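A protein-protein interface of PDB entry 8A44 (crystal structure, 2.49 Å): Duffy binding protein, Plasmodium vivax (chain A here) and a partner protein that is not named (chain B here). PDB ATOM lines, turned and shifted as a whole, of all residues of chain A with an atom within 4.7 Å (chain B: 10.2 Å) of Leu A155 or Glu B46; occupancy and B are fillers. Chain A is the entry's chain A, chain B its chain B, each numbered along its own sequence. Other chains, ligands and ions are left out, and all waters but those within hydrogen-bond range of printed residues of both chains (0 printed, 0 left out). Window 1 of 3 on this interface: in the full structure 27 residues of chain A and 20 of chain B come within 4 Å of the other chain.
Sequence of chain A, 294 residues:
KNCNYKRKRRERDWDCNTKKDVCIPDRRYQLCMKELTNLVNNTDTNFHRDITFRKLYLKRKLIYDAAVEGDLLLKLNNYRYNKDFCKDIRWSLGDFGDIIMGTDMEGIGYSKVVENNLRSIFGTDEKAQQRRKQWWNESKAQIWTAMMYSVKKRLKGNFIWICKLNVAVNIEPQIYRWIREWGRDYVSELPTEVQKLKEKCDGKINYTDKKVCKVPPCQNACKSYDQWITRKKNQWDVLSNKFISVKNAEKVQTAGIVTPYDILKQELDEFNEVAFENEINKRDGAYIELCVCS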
ATOM      1  N   TYR A  79      22.605  17.428   9.678  1.00  0.00           N
ATOM      2  CA  TYR A  79      23.519  18.283  10.429  1.00  0.00           C
ATOM      3  C   TYR A  79      23.249  18.242  11.932  1.00  0.00           C
ATOM      4  O   TYR A  79      23.477  19.225  12.641  1.00  0.00           O
ATOM      5  CB  TYR A  79      23.486  19.716   9.893  1.00  0.00           C
ATOM      6  CG  TYR A  79      23.950  19.770   8.460  1.00  0.00           C
ATOM      7  CD1 TYR A  79      25.300  19.904   8.160  1.00  0.00           C
ATOM      8  CD2 TYR A  79      23.050  19.643   7.406  1.00  0.00           C
ATOM      9  CE1 TYR A  79      25.737  19.933   6.852  1.00  0.00           C
ATOM     10  CE2 TYR A  79      23.480  19.675   6.089  1.00  0.00           C
ATOM     11  CZ  TYR A  79      24.828  19.821   5.819  1.00  0.00           C
ATOM     12  OH  TYR A  79      25.286  19.858   4.517  1.00  0.00           O
ATOM     13  N   ARG A  80      22.794  17.094  12.429  1.00  0.00           N
ATOM     14  CA  ARG A  80      22.632  16.864  13.861  1.00  0.00           C
ATOM     15  C   ARG A  80      23.823  16.064  14.376  1.00  0.00           C
ATOM     16  O   ARG A  80      24.114  14.972  13.868  1.00  0.00           O
ATOM     17  CB  ARG A  80      21.328  16.123  14.175  1.00  0.00           C
ATOM     18  CG  ARG A  80      20.066  16.743  13.586  1.00  0.00           C
ATOM     19  CD  ARG A  80      19.805  18.154  14.102  1.00  0.00           C
ATOM     20  NE  ARG A  80      19.817  18.240  15.559  1.00  0.00           N
ATOM     21  CZ  ARG A  80      19.657  19.364  16.248  1.00  0.00           C
ATOM     22  NH1 ARG A  80      19.408  20.518  15.645  1.00  0.00           N
ATOM     23  NH2 ARG A  80      19.735  19.329  17.576  1.00  0.00           N
ATOM     24  N   TYR A  81      24.495  16.604  15.388  1.00  0.00           N
ATOM     25  CA  TYR A  81      25.586  15.924  16.077  1.00  0.00           C
ATOM     26  C   TYR A  81      24.978  15.186  17.264  1.00  0.00           C
ATOM     27  O   TYR A  81      24.910  15.704  18.380  1.00  0.00           O
ATOM     28  CB  TYR A  81      26.645  16.935  16.499  1.00  0.00           C
ATOM     29  CG  TYR A  81      27.864  16.372  17.195  1.00  0.00           C
ATOM     30  CD1 TYR A  81      28.406  15.145  16.833  1.00  0.00           C
ATOM     31  CD2 TYR A  81      28.503  17.097  18.190  1.00  0.00           C
ATOM     32  CE1 TYR A  81      29.538  14.648  17.476  1.00  0.00           C
ATOM     33  CE2 TYR A  81      29.631  16.612  18.830  1.00  0.00           C
ATOM     34  CZ  TYR A  81      30.138  15.391  18.474  1.00  0.00           C
ATOM     35  OH  TYR A  81      31.252  14.919  19.113  1.00  0.00           O
ATOM     36  N   VAL A 151      32.154  17.887  11.716  1.00  0.00           N
ATOM     37  CA  VAL A 151      31.484  18.322  12.949  1.00  0.00           C
ATOM     38  C   VAL A 151      32.368  19.280  13.738  1.00  0.00           C
ATOM     39  O   VAL A 151      31.934  20.372  14.136  1.00  0.00           O
ATOM     40  CB  VAL A 151      31.059  17.122  13.816  1.00  0.00           C
ATOM     41  CG1 VAL A 151      29.751  16.566  13.347  1.00  0.00           C
ATOM     42  CG2 VAL A 151      32.117  16.047  13.802  1.00  0.00           C
ATOM     43  N   LYS A 152      33.620  18.882  13.979  1.00  0.00           N
ATOM     44  CA  LYS A 152      34.558  19.729  14.706  1.00  0.00           C
ATOM     45  C   LYS A 152      34.627  21.124  14.099  1.00  0.00           C
ATOM     46  O   LYS A 152      34.466  22.125  14.803  1.00  0.00           O
ATOM     47  CB  LYS A 152      35.940  19.076  14.716  1.00  0.00           C
ATOM     48  CG  LYS A 152      36.530  18.819  16.091  1.00  0.00           C
ATOM     49  CD  LYS A 152      38.045  18.759  15.999  1.00  0.00           C
ATOM     50  CE  LYS A 152      38.664  18.328  17.317  1.00  0.00           C
ATOM     51  NZ  LYS A 152      40.073  18.845  17.520  1.00  0.00           N
ATOM     52  N   LYS A 153      34.842  21.205  12.781  1.00  0.00           N
ATOM     53  CA  LYS A 153      35.021  22.501  12.132  1.00  0.00           C
ATOM     54  C   LYS A 153      33.779  23.368  12.270  1.00  0.00           C
ATOM     55  O   LYS A 153      33.879  24.572  12.540  1.00  0.00           O
ATOM     56  CB  LYS A 153      35.363  22.310  10.652  1.00  0.00           C
ATOM     57  CG  LYS A 153      35.746  23.587   9.936  1.00  0.00           C
ATOM     58  CD  LYS A 153      37.194  23.930  10.212  1.00  0.00           C
ATOM     59  CE  LYS A 153      37.674  25.055   9.304  1.00  0.00           C
ATOM     60  NZ  LYS A 153      39.051  25.443   9.668  1.00  0.00           N
ATOM     61  N   ARG A 154      32.601  22.766  12.103  1.00  0.00           N
ATOM     62  CA  ARG A 154      31.349  23.514  12.126  1.00  0.00           C
ATOM     63  C   ARG A 154      31.005  24.015  13.526  1.00  0.00           C
ATOM     64  O   ARG A 154      30.596  25.172  13.691  1.00  0.00           O
ATOM     65  CB  ARG A 154      30.228  22.638  11.574  1.00  0.00           C
ATOM     66  CG  ARG A 154      30.449  22.270  10.137  1.00  0.00           C
ATOM     67  CD  ARG A 154      29.255  21.589   9.553  1.00  0.00           C
ATOM     68  NE  ARG A 154      29.590  21.043   8.246  1.00  0.00           N
ATOM     69  CZ  ARG A 154      28.984  21.386   7.117  1.00  0.00           C
ATOM     70  NH1 ARG A 154      27.965  22.237   7.110  1.00  0.00           N
ATOM     71  NH2 ARG A 154      29.412  20.864   5.964  1.00  0.00           N
ATOM     72  N   LEU A 155      31.155  23.164  14.547  1.00  0.00           N
ATOM     73  CA  LEU A 155      30.784  23.567  15.901  1.00  0.00           C
ATOM     74  C   LEU A 155      31.760  24.577  16.500  1.00  0.00           C
ATOM     75  O   LEU A 155      31.365  25.340  17.392  1.00  0.00           O
ATOM     76  CB  LEU A 155      30.665  22.341  16.807  1.00  0.00           C
ATOM     77  CG  LEU A 155      29.264  21.711  16.848  1.00  0.00           C
ATOM     78  CD1 LEU A 155      28.787  21.272  15.459  1.00  0.00           C
ATOM     79  CD2 LEU A 155      29.213  20.544  17.824  1.00  0.00           C
ATOM     80  N   LYS A 156      33.007  24.614  16.020  1.00  0.00           N
ATOM     81  CA  LYS A 156      33.991  25.584  16.493  1.00  0.00           C
ATOM     82  C   LYS A 156      34.068  25.541  18.012  1.00  0.00           C
ATOM     83  O   LYS A 156      34.305  24.478  18.592  1.00  0.00           O
ATOM     84  CB  LYS A 156      33.655  27.004  16.005  1.00  0.00           C
ATOM     85  CG  LYS A 156      33.334  27.095  14.512  1.00  0.00           C
ATOM     86  CD  LYS A 156      33.952  28.315  13.840  1.00  0.00           C
ATOM     87  CE  LYS A 156      35.317  27.963  13.209  1.00  0.00           C
ATOM     88  NZ  LYS A 156      35.274  27.241  11.886  1.00  0.00           N
ATOM     89  N   GLY A 157      33.832  26.683  18.664  1.00  0.00           N
ATOM     90  CA  GLY A 157      34.001  26.774  20.104  1.00  0.00           C
ATOM     91  C   GLY A 157      33.056  25.903  20.905  1.00  0.00           C
ATOM     92  O   GLY A 157      33.339  25.606  22.070  1.00  0.00           O
ATOM     93  N   ASN A 158      31.947  25.474  20.309  1.00  0.00           N
ATOM     94  CA  ASN A 158      30.933  24.698  21.011  1.00  0.00           C
ATOM     95  C   ASN A 158      31.124  23.192  20.895  1.00  0.00           C
ATOM     96  O   ASN A 158      30.306  22.438  21.428  1.00  0.00           O
ATOM     97  CB  ASN A 158      29.547  25.067  20.482  1.00  0.00           C
ATOM     98  CG  ASN A 158      29.364  26.561  20.356  1.00  0.00           C
ATOM     99  OD1 ASN A 158      29.504  27.299  21.336  1.00  0.00           O
ATOM    100  ND2 ASN A 158      29.077  27.024  19.140  1.00  0.00           N
ATOM    101  N   PHE A 159      32.164  22.731  20.214  1.00  0.00           N
ATOM    102  CA  PHE A 159      32.333  21.299  20.032  1.00  0.00           C
ATOM    103  C   PHE A 159      32.545  20.601  21.373  1.00  0.00           C
ATOM    104  O   PHE A 159      33.141  21.148  22.306  1.00  0.00           O
ATOM    105  CB  PHE A 159      33.509  21.007  19.100  1.00  0.00           C
ATOM    106  CG  PHE A 159      33.697  19.548  18.807  1.00  0.00           C
ATOM    107  CD1 PHE A 159      32.817  18.883  17.967  1.00  0.00           C
ATOM    108  CD2 PHE A 159      34.748  18.843  19.375  1.00  0.00           C
ATOM    109  CE1 PHE A 159      32.984  17.536  17.693  1.00  0.00           C
ATOM    110  CE2 PHE A 159      34.924  17.500  19.111  1.00  0.00           C
ATOM    111  CZ  PHE A 159      34.044  16.842  18.268  1.00  0.00           C
ATOM    112  N   PHE B  36      38.745  20.313  24.290  1.00  0.00           N
ATOM    113  CA  PHE B  36      37.309  20.233  24.306  1.00  0.00           C
ATOM    114  C   PHE B  36      36.863  19.225  25.357  1.00  0.00           C
ATOM    115  O   PHE B  36      37.575  18.270  25.643  1.00  0.00           O
ATOM    116  CB  PHE B  36      36.769  19.802  22.941  1.00  0.00           C
ATOM    117  CG  PHE B  36      37.012  20.795  21.850  1.00  0.00           C
ATOM    118  CD1 PHE B  36      36.147  21.871  21.670  1.00  0.00           C
ATOM    119  CD2 PHE B  36      38.091  20.653  20.996  1.00  0.00           C
ATOM    120  CE1 PHE B  36      36.371  22.795  20.656  1.00  0.00           C
ATOM    121  CE2 PHE B  36      38.316  21.567  19.985  1.00  0.00           C
ATOM    122  CZ  PHE B  36      37.459  22.643  19.816  1.00  0.00           C
ATOM    123  N   PRO B  37      35.674  19.392  25.940  1.00  0.00           N
ATOM    124  CA  PRO B  37      35.219  18.493  27.008  1.00  0.00           C
ATOM    125  C   PRO B  37      34.382  17.328  26.493  1.00  0.00           C
ATOM    126  O   PRO B  37      33.922  17.307  25.352  1.00  0.00           O
ATOM    127  CB  PRO B  37      34.360  19.421  27.901  1.00  0.00           C
ATOM    128  CG  PRO B  37      33.896  20.547  26.978  1.00  0.00           C
ATOM    129  CD  PRO B  37      34.597  20.358  25.611  1.00  0.00           C
ATOM    130  N   GLY B  39      31.215  14.983  26.110  1.00  0.00           N
ATOM    131  CA  GLY B  39      29.769  15.223  26.082  1.00  0.00           C
ATOM    132  C   GLY B  39      29.047  13.941  26.420  1.00  0.00           C
ATOM    133  O   GLY B  39      29.626  12.865  26.215  1.00  0.00           O
ATOM    134  N   ALA B  43      23.412  13.647  24.027  1.00  0.00           N
ATOM    135  CA  ALA B  43      23.377  15.061  23.609  1.00  0.00           C
ATOM    136  C   ALA B  43      22.976  15.161  22.141  1.00  0.00           C
ATOM    137  O   ALA B  43      22.968  14.133  21.451  1.00  0.00           O
ATOM    138  CB  ALA B  43      24.710  15.701  23.865  1.00  0.00           C
ATOM    139  N   ASN B  44      22.685  16.373  21.689  1.00  0.00           N
ATOM    140  CA  ASN B  44      22.197  16.583  20.331  1.00  0.00           C
ATOM    141  C   ASN B  44      22.393  18.063  19.979  1.00  0.00           C
ATOM    142  O   ASN B  44      21.607  18.904  20.424  1.00  0.00           O
ATOM    143  CB  ASN B  44      20.737  16.181  20.244  1.00  0.00           C
ATOM    144  CG  ASN B  44      20.277  15.978  18.828  1.00  0.00           C
ATOM    145  OD1 ASN B  44      20.343  16.884  18.003  1.00  0.00           O
ATOM    146  ND2 ASN B  44      19.745  14.797  18.553  1.00  0.00           N
ATOM    147  N   LEU B  45      23.397  18.320  19.137  1.00  0.00           N
ATOM    148  CA  LEU B  45      23.713  19.714  18.743  1.00  0.00           C
ATOM    149  C   LEU B  45      23.458  19.906  17.245  1.00  0.00           C
ATOM    150  O   LEU B  45      22.921  18.973  16.567  1.00  0.00           O
ATOM    151  CB  LEU B  45      25.183  19.996  19.070  1.00  0.00           C
ATOM    152  CG  LEU B  45      25.553  19.975  20.553  1.00  0.00           C
ATOM    153  CD1 LEU B  45      24.399  20.464  21.414  1.00  0.00           C
ATOM    154  CD2 LEU B  45      25.995  18.586  20.985  1.00  0.00           C
ATOM    155  N   GLU B  46      23.864  21.072  16.742  1.00  0.00           N
ATOM    156  CA  GLU B  46      23.597  21.374  15.315  1.00  0.00           C
ATOM    157  C   GLU B  46      24.847  21.954  14.647  1.00  0.00           C
ATOM    158  O   GLU B  46      25.634  22.624  15.344  1.00  0.00           O
ATOM    159  CB  GLU B  46      22.386  22.299  15.204  1.00  0.00           C
ATOM    160  CG  GLU B  46      21.714  22.197  13.842  1.00  0.00           C
ATOM    161  CD  GLU B  46      20.301  22.750  13.784  1.00  0.00           C
ATOM    162  OE1 GLU B  46      19.422  22.063  13.227  1.00  0.00           O
ATOM    163  OE2 GLU B  46      20.083  23.865  14.299  1.00  0.00           O
ATOM    164  N   ALA B  47      25.013  21.698  13.350  1.00  0.00           N
ATOM    165  CA  ALA B  47      26.164  22.174  12.562  1.00  0.00           C
ATOM    166  C   ALA B  47      26.606  23.614  12.900  1.00  0.00           C
ATOM    167  O   ALA B  47      26.766  24.470  12.024  1.00  0.00           O
ATOM    168  CB  ALA B  47      25.863  22.061  11.077  1.00  0.00           C
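O of Tyr A79 touches O of Leu B45, 3.97 Å away. Tyr A79 touches Glu B46 (O to CA, 3.4 Å). Ala B43 touches Tyr A81 (O to O, 3.96 Å). Tyr A81 touches Asn B44. CB of Ala B47 touches CD of Arg A154 (3.7 Å). CD1 of Leu A155 touches O of Glu B46, at 3.4 Å. Phe B36 touches Lys A156 (CE1 to O, 3.4 Å). Phe A159 touches Phe B36. CD of Pro B37 touches O of Phe A159 (3.7 Å).
O of Leu A155 sits at hydrogen-bond distance from ND2 of Asn A158 (3.3 Å). The backbone carbonyl oxygen of Lys A153 lies within hydrogen-bond range of the side-chain amino group of Lys A156, 3.1 Å away.
Printed residues of chain B that touch a printed residue of chain A: Phe B36, Pro B37, Ala B43, Asn B44, Leu B45, Glu B46 and Ala B47. Hydrophobic or aromatic side chains of chain B within 4 Å of the printed part of chain A: Phe B36, Pro B37 and Ala B47. Of the 12 printed residues of chain A, 7 touch a printed residue of chain B. Hydrophobic or aromatic side chains of chain A that line the printed part of chain B: Tyr A79, Leu A155 and Phe A159. Among the printed residues, 14 pairs touch across the chains. Among the printed residues, Asp or Glu carboxylates within 4 Å of a Lys or Arg side-chain nitrogen of the other chain: Arg A80 with Glu B46 (2.9 Å).
Printed residues of chain B within 4 Å of Tyr A79: Leu B45 (3.97 Å), Glu B46 (3.4 Å) and Ala B47 (3.0 Å). Of the printed residues of chain B, Tyr A81 touches Ala B43, Asn B44 and Leu B45. Val A151 touches none of the printed residues of chain B. Printed residues of chain B within 4 Å of Leu A155: Glu B46. No residue of chain B comes within 4 Å of Gly A157. No residue of chain B comes within 4 Å of Asn A158. Of the printed residues of chain A, Ala B47 touches Tyr A79 and Arg A154. The nearest printed residue of chain A that does not touch Ala B47 is Leu A155 (4.01 Å).
The backbone carbonyl oxygen of Leu B45 lies close to the guanidinium group of Arg A80 (3.3 Å). NH2 of Arg A80 sits at hydrogen-bond distance from OD1 of Asn B44. The backbone carbonyl oxygen (O) of Tyr A79 sits at hydrogen-bond distance from the backbone NH (N) of Ala B47, 3.0 Å away. The guanidinium group (NH1) of Arg A80 is in salt-bridge range of the side-chain carboxylate (OE1) of Glu B46, at 2.9 Å. The backbone NH of Tyr A81 lies within hydrogen-bond range of the backbone carbonyl oxygen of Leu B45 (3.1 Å).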
